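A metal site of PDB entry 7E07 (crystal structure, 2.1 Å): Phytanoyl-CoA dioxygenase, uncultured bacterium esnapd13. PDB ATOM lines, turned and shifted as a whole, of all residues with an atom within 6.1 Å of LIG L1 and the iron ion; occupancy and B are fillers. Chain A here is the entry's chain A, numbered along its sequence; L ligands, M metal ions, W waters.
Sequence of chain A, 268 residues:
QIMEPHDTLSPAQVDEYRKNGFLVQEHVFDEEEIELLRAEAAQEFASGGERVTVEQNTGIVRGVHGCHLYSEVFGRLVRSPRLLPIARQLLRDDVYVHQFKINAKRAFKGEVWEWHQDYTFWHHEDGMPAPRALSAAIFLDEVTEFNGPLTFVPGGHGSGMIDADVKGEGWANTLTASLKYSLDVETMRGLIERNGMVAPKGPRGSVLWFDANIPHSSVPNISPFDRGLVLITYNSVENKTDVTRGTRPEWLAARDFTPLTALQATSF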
ATOM      1  N   GLN A  99      11.195  12.049   9.416  1.00  0.00           N
ATOM      2  CA  GLN A  99      12.455  12.205   8.704  1.00  0.00           C
ATOM      3  C   GLN A  99      13.113  10.882   8.542  1.00  0.00           C
ATOM      4  O   GLN A  99      12.937   9.960   9.363  1.00  0.00           O
ATOM      5  CB  GLN A  99      13.353  13.168   9.549  1.00  0.00           C
ATOM      6  CG  GLN A  99      14.740  13.481   9.064  1.00  0.00           C
ATOM      7  CD  GLN A  99      15.424  14.503   9.975  1.00  0.00           C
ATOM      8  OE1 GLN A  99      16.276  14.150  10.779  1.00  0.00           O
ATOM      9  NE2 GLN A  99      15.041  15.768   9.863  1.00  0.00           N
ATOM     10  N   LYS A 101      16.996   9.517   7.241  1.00  0.00           N
ATOM     11  CA  LYS A 101      18.349   9.805   6.716  1.00  0.00           C
ATOM     12  C   LYS A 101      19.296   8.649   6.875  1.00  0.00           C
ATOM     13  O   LYS A 101      19.127   7.774   7.755  1.00  0.00           O
ATOM     14  CB  LYS A 101      18.888  11.112   7.342  1.00  0.00           C
ATOM     15  CG  LYS A 101      19.180  10.974   8.834  1.00  0.00           C
ATOM     16  CD  LYS A 101      19.243  12.320   9.573  1.00  0.00           C
ATOM     17  CE  LYS A 101      19.113  12.152  11.087  1.00  0.00           C
ATOM     18  NZ  LYS A 101      17.680  12.135  11.601  1.00  0.00           N
ATOM     19  N   ASN A 103      23.378   8.205   7.353  1.00  0.00           N
ATOM     20  CA  ASN A 103      24.663   8.850   7.696  1.00  0.00           C
ATOM     21  C   ASN A 103      25.795   7.774   7.565  1.00  0.00           C
ATOM     22  O   ASN A 103      25.752   6.743   8.303  1.00  0.00           O
ATOM     23  CB  ASN A 103      24.624   9.407   9.145  1.00  0.00           C
ATOM     24  CG  ASN A 103      23.793  10.704   9.258  1.00  0.00           C
ATOM     25  OD1 ASN A 103      23.340  11.233   8.252  1.00  0.00           O
ATOM     26  ND2 ASN A 103      23.603  11.188  10.472  1.00  0.00           N
ATOM     27  N   LYS A 105      29.617   6.934   7.904  1.00  0.00           N
ATOM     28  CA  LYS A 105      30.798   7.383   8.681  1.00  0.00           C
ATOM     29  C   LYS A 105      31.852   6.445   8.197  1.00  0.00           C
ATOM     30  O   LYS A 105      31.977   5.302   8.677  1.00  0.00           O
ATOM     31  CB  LYS A 105      30.419   7.302  10.159  1.00  0.00           C
ATOM     32  CG  LYS A 105      31.423   7.870  11.132  1.00  0.00           C
ATOM     33  CD  LYS A 105      30.771   8.306  12.414  1.00  0.00           C
ATOM     34  CE  LYS A 105      30.711   9.800  12.515  1.00  0.00           C
ATOM     35  NZ  LYS A 105      30.417  10.203  13.906  1.00  0.00           N
ATOM     36  N   TRP A 113      30.028  15.041  15.150  1.00  0.00           N
ATOM     37  CA  TRP A 113      28.683  15.660  15.365  1.00  0.00           C
ATOM     38  C   TRP A 113      28.585  16.174  16.779  1.00  0.00           C
ATOM     39  O   TRP A 113      28.633  15.407  17.716  1.00  0.00           O
ATOM     40  CB  TRP A 113      27.568  14.658  15.113  1.00  0.00           C
ATOM     41  CG  TRP A 113      27.394  14.222  13.682  1.00  0.00           C
ATOM     42  CD1 TRP A 113      28.206  13.351  13.005  1.00  0.00           C
ATOM     43  CD2 TRP A 113      26.366  14.615  12.751  1.00  0.00           C
ATOM     44  NE1 TRP A 113      27.750  13.185  11.696  1.00  0.00           N
ATOM     45  CE2 TRP A 113      26.621  13.935  11.522  1.00  0.00           C
ATOM     46  CE3 TRP A 113      25.257  15.466  12.819  1.00  0.00           C
ATOM     47  CZ2 TRP A 113      25.785  14.092  10.383  1.00  0.00           C
ATOM     48  CZ3 TRP A 113      24.458  15.658  11.653  1.00  0.00           C
ATOM     49  CH2 TRP A 113      24.732  14.963  10.468  1.00  0.00           C
ATOM     50  N   HIS A 116      23.758  17.474  20.762  1.00  0.00           N
ATOM     51  CA  HIS A 116      22.480  18.047  20.352  1.00  0.00           C
ATOM     52  C   HIS A 116      21.315  17.128  20.706  1.00  0.00           C
ATOM     53  O   HIS A 116      21.483  15.936  21.095  1.00  0.00           O
ATOM     54  CB  HIS A 116      22.465  18.411  18.864  1.00  0.00           C
ATOM     55  CG  HIS A 116      22.421  17.241  17.949  1.00  0.00           C
ATOM     56  ND1 HIS A 116      23.537  16.511  17.623  1.00  0.00           N
ATOM     57  CD2 HIS A 116      21.381  16.652  17.303  1.00  0.00           C
ATOM     58  CE1 HIS A 116      23.193  15.509  16.836  1.00  0.00           C
ATOM     59  NE2 HIS A 116      21.894  15.585  16.618  1.00  0.00           N
ATOM     60  N   GLN A 117      20.135  17.753  20.728  1.00  0.00           N
ATOM     61  CA  GLN A 117      18.863  17.075  20.903  1.00  0.00           C
ATOM     62  C   GLN A 117      18.155  17.217  19.567  1.00  0.00           C
ATOM     63  O   GLN A 117      18.085  18.340  19.000  1.00  0.00           O
ATOM     64  CB  GLN A 117      18.074  17.686  22.017  1.00  0.00           C
ATOM     65  CG  GLN A 117      18.658  17.399  23.345  1.00  0.00           C
ATOM     66  CD  GLN A 117      18.000  18.251  24.429  1.00  0.00           C
ATOM     67  OE1 GLN A 117      18.112  19.476  24.377  1.00  0.00           O
ATOM     68  NE2 GLN A 117      17.328  17.632  25.405  1.00  0.00           N
ATOM     69  N   ASP A 118      17.718  16.111  18.978  1.00  0.00           N
ATOM     70  CA  ASP A 118      17.066  16.195  17.644  1.00  0.00           C
ATOM     71  C   ASP A 118      15.802  17.057  17.691  1.00  0.00           C
ATOM     72  O   ASP A 118      15.482  17.724  16.756  1.00  0.00           O
ATOM     73  CB  ASP A 118      16.637  14.826  17.121  1.00  0.00           C
ATOM     74  CG  ASP A 118      17.808  13.935  16.706  1.00  0.00           C
ATOM     75  OD1 ASP A 118      18.942  14.441  16.474  1.00  0.00           O
ATOM     76  OD2 ASP A 118      17.563  12.702  16.641  1.00  0.00           O
ATOM     77  N   GLY A 148      33.096   5.546  15.699  1.00  0.00           N
ATOM     78  CA  GLY A 148      32.301   6.735  15.863  1.00  0.00           C
ATOM     79  C   GLY A 148      30.853   6.446  16.234  1.00  0.00           C
ATOM     80  O   GLY A 148      29.999   6.944  15.572  1.00  0.00           O
ATOM     81  N   PRO A 149      30.603   5.599  17.237  1.00  0.00           N
ATOM     82  CA  PRO A 149      29.238   5.295  17.659  1.00  0.00           C
ATOM     83  C   PRO A 149      28.470   6.516  18.117  1.00  0.00           C
ATOM     84  O   PRO A 149      29.028   7.458  18.690  1.00  0.00           O
ATOM     85  CB  PRO A 149      29.452   4.355  18.865  1.00  0.00           C
ATOM     86  CG  PRO A 149      30.803   4.806  19.422  1.00  0.00           C
ATOM     87  CD  PRO A 149      31.585   5.064  18.185  1.00  0.00           C
ATOM     88  N   LEU A 150      27.164   6.482  17.934  1.00  0.00           N
ATOM     89  CA  LEU A 150      26.341   7.466  18.609  1.00  0.00           C
ATOM     90  C   LEU A 150      26.549   7.345  20.108  1.00  0.00           C
ATOM     91  O   LEU A 150      26.521   6.237  20.665  1.00  0.00           O
ATOM     92  CB  LEU A 150      24.851   7.207  18.279  1.00  0.00           C
ATOM     93  CG  LEU A 150      24.099   8.109  17.357  1.00  0.00           C
ATOM     94  CD1 LEU A 150      24.990   9.016  16.546  1.00  0.00           C
ATOM     95  CD2 LEU A 150      23.272   7.267  16.410  1.00  0.00           C
ATOM     96  N   PHE A 210      16.057   5.477  19.801  1.00  0.00           N
ATOM     97  CA  PHE A 210      16.351   6.572  20.720  1.00  0.00           C
ATOM     98  C   PHE A 210      15.374   7.728  20.688  1.00  0.00           C
ATOM     99  O   PHE A 210      14.848   8.098  19.637  1.00  0.00           O
ATOM    100  CB  PHE A 210      17.794   7.060  20.613  1.00  0.00           C
ATOM    101  CG  PHE A 210      18.159   7.709  19.334  1.00  0.00           C
ATOM    102  CD1 PHE A 210      18.158   9.063  19.203  1.00  0.00           C
ATOM    103  CD2 PHE A 210      18.729   6.980  18.318  1.00  0.00           C
ATOM    104  CE1 PHE A 210      18.617   9.662  18.072  1.00  0.00           C
ATOM    105  CE2 PHE A 210      19.137   7.569  17.148  1.00  0.00           C
ATOM    106  CZ  PHE A 210      19.084   8.914  17.014  1.00  0.00           C
ATOM    107  N   HIS A 216      22.735  13.712  22.195  1.00  0.00           N
ATOM    108  CA  HIS A 216      23.705  12.751  21.659  1.00  0.00           C
ATOM    109  C   HIS A 216      24.766  13.404  20.860  1.00  0.00           C
ATOM    110  O   HIS A 216      24.632  14.554  20.317  1.00  0.00           O
ATOM    111  CB  HIS A 216      23.026  11.596  20.826  1.00  0.00           C
ATOM    112  CG  HIS A 216      22.128  12.088  19.713  1.00  0.00           C
ATOM    113  ND1 HIS A 216      20.890  12.595  19.958  1.00  0.00           N
ATOM    114  CD2 HIS A 216      22.314  12.186  18.380  1.00  0.00           C
ATOM    115  CE1 HIS A 216      20.331  12.952  18.815  1.00  0.00           C
ATOM    116  NE2 HIS A 216      21.202  12.779  17.849  1.00  0.00           N
ATOM    117  N   SER A 217      25.802  12.611  20.683  1.00  0.00           N
ATOM    118  CA  SER A 217      27.001  13.062  19.938  1.00  0.00           C
ATOM    119  C   SER A 217      27.728  11.911  19.236  1.00  0.00           C
ATOM    120  O   SER A 217      27.512  10.748  19.569  1.00  0.00           O
ATOM    121  CB  SER A 217      28.006  13.694  20.943  1.00  0.00           C
ATOM    122  OG  SER A 217      29.006  14.410  20.214  1.00  0.00           O
ATOM    123  N   SER A 218      28.684  12.249  18.384  1.00  0.00           N
ATOM    124  CA  SER A 218      29.634  11.202  17.919  1.00  0.00           C
ATOM    125  C   SER A 218      30.939  11.761  17.347  1.00  0.00           C
ATOM    126  O   SER A 218      30.980  12.846  16.856  1.00  0.00           O
ATOM    127  CB  SER A 218      28.985  10.369  16.818  1.00  0.00           C
ATOM    128  OG  SER A 218      28.752  11.196  15.695  1.00  0.00           O
ATOM    129  N   ARG A 227      30.830   2.758   9.314  1.00  0.00           N
ATOM    130  CA  ARG A 227      29.692   2.775  10.249  1.00  0.00           C
ATOM    131  C   ARG A 227      28.446   3.424   9.566  1.00  0.00           C
ATOM    132  O   ARG A 227      28.116   4.532   9.879  1.00  0.00           O
ATOM    133  CB  ARG A 227      30.083   3.484  11.566  1.00  0.00           C
ATOM    134  CG  ARG A 227      29.051   3.402  12.661  1.00  0.00           C
ATOM    135  CD  ARG A 227      28.695   4.729  13.288  1.00  0.00           C
ATOM    136  NE  ARG A 227      27.982   5.586  12.369  1.00  0.00           N
ATOM    137  CZ  ARG A 227      27.480   6.796  12.654  1.00  0.00           C
ATOM    138  NH1 ARG A 227      27.584   7.351  13.847  1.00  0.00           N
ATOM    139  NH2 ARG A 227      26.872   7.478  11.710  1.00  0.00           N
ATOM    140  N   LEU A 229      24.548   4.080   9.185  1.00  0.00           N
ATOM    141  CA  LEU A 229      23.337   4.091  10.024  1.00  0.00           C
ATOM    142  C   LEU A 229      22.181   4.510   9.088  1.00  0.00           C
ATOM    143  O   LEU A 229      22.240   5.541   8.435  1.00  0.00           O
ATOM    144  CB  LEU A 229      23.489   5.084  11.153  1.00  0.00           C
ATOM    145  CG  LEU A 229      24.440   4.678  12.283  1.00  0.00           C
ATOM    146  CD1 LEU A 229      24.277   5.617  13.425  1.00  0.00           C
ATOM    147  CD2 LEU A 229      24.196   3.269  12.842  1.00  0.00           C
ATOM    148  N   LEU A 231      18.709   5.922   9.729  1.00  0.00           N
ATOM    149  CA  LEU A 231      17.922   6.569  10.764  1.00  0.00           C
ATOM    150  C   LEU A 231      16.489   6.920  10.287  1.00  0.00           C
ATOM    151  O   LEU A 231      16.315   7.817   9.459  1.00  0.00           O
ATOM    152  CB  LEU A 231      18.625   7.844  11.240  1.00  0.00           C
ATOM    153  CG  LEU A 231      19.880   7.473  12.093  1.00  0.00           C
ATOM    154  CD1 LEU A 231      21.112   7.922  11.379  1.00  0.00           C
ATOM    155  CD2 LEU A 231      19.823   8.147  13.464  1.00  0.00           C
HETATM  156  C1  LIG L   1      21.704  13.308  13.440  1.00  0.00           C
HETATM  157  O1  LIG L   1      20.792  14.003  14.032  1.00  0.00           O
HETATM  158  O2  LIG L   1      21.878  13.274  12.181  1.00  0.00           O
HETATM  159  C2  LIG L   1      22.625  12.525  14.296  1.00  0.00           C
HETATM  160  O3  LIG L   1      22.612  12.698  15.476  1.00  0.00           O
HETATM  161  C3  LIG L   1      23.454  11.383  13.792  1.00  0.00           C
HETATM  162  C4  LIG L   1      24.968  11.556  13.900  1.00  0.00           C
HETATM  163  C5  LIG L   1      25.745  10.316  13.477  1.00  0.00           C
HETATM  164  O4  LIG L   1      26.751   9.939  14.150  1.00  0.00           O
HETATM  165  O5  LIG L   1      25.396   9.677  12.428  1.00  0.00           O
HETATM  166  N1  LG2 L   2      20.002  17.185  11.932  1.00  0.00           N
HETATM  167  C1  LG2 L   2      18.603  16.660  11.917  1.00  0.00           C
HETATM  168  C2  LG2 L   2      17.609  17.737  11.489  1.00  0.00           C
HETATM  169  O1  LG2 L   2      16.412  17.538  11.590  1.00  0.00           O
HETATM  170  C3  LG2 L   2      18.353  16.255  13.367  1.00  0.00           C
HETATM  171  C4  LG2 L   2      19.386  17.017  14.177  1.00  0.00           C
HETATM  172  C5  LG2 L   2      20.585  17.158  13.292  1.00  0.00           C
HETATM  173  O2  LG2 L   2      17.982  18.823  11.051  1.00  0.00           O
HETATM  174 FE    FE M   1      20.832  13.673  15.953  1.00  0.00          FE
HETATM  175  O   HOH W   1      20.888  15.216  10.382  1.00  0.00           O
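An oxygen (O4) of LIG L1 is in salt-bridge range of the guanidinium group (NH1) of Arg 227 (2.7 Å).
The side-chain hydroxyl of Ser 218 is in hydrogen-bond range of an oxygen (O4) of LIG L1.
O5 of LIG L1 sits at hydrogen-bond distance from ND2 of Asn 103 (3.1 Å).
The side-chain amino group of Lys 105 is in salt-bridge range of an oxygen (O4) of LIG L1.
The side-chain amide nitrogen (NE2) of Gln 99 lies within hydrogen-bond range of an oxygen (O1) of LG2 L2 (2.8 Å).
The iron ion is bound by O1 of LIG L1 (1.9 Å), O3 of LIG L1 (2.1 Å), OD1 of Asp 118 (2.1 Å), NE2 of His 216 (2.1 Å) and NE2 of His 116 (2.3 Å).
The backbone NH (N) of Arg 227 lies within hydrogen-bond range of the backbone carbonyl oxygen (O) of Lys 105 (2.9 Å).
The backbone carbonyl oxygen of Gly 148 is in hydrogen-bond range of the guanidinium group of Arg 227 (3.0 Å).
O of Ser 218 sits at hydrogen-bond distance from N of Trp 113, at 2.9 Å.
OG of Ser 218 sits at hydrogen-bond distance from NZ of Lys 105 (2.6 Å).
The backbone carbonyl oxygen (O) of Asn 103 sits at hydrogen-bond distance from the backbone NH (N) of Leu 229 (3.1 Å).
The backbone NH of Leu 231 sits at hydrogen-bond distance from the backbone carbonyl oxygen of Lys 101 (2.7 Å).
NZ of Lys 101 sits at hydrogen-bond distance from OE1 of Gln 99 (2.6 Å).
The backbone carbonyl oxygen of Trp 113 sits at hydrogen-bond distance from the side-chain hydroxyl of Ser 217 (2.7 Å).
Of the 18 residues printed, 3 come within 4 Å of the iron ion.
Residues that only touch LIG L1: Leu 150 (3.1 Å), Lys 101 (3.2 Å) and Trp 113 (3.6 Å).
Hydrophobic or aromatic side chains within 4 Å of LIG L1: Trp 113, His 116, Leu 150 and His 216.
The nearest printed residue that does not touch LIG L1 is Leu 229 (4.3 Å).
Water W1 lies within hydrogen-bond range of N1 of LG2 L2 (2.7 Å) and O2 of LIG L1 (2.8 Å).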
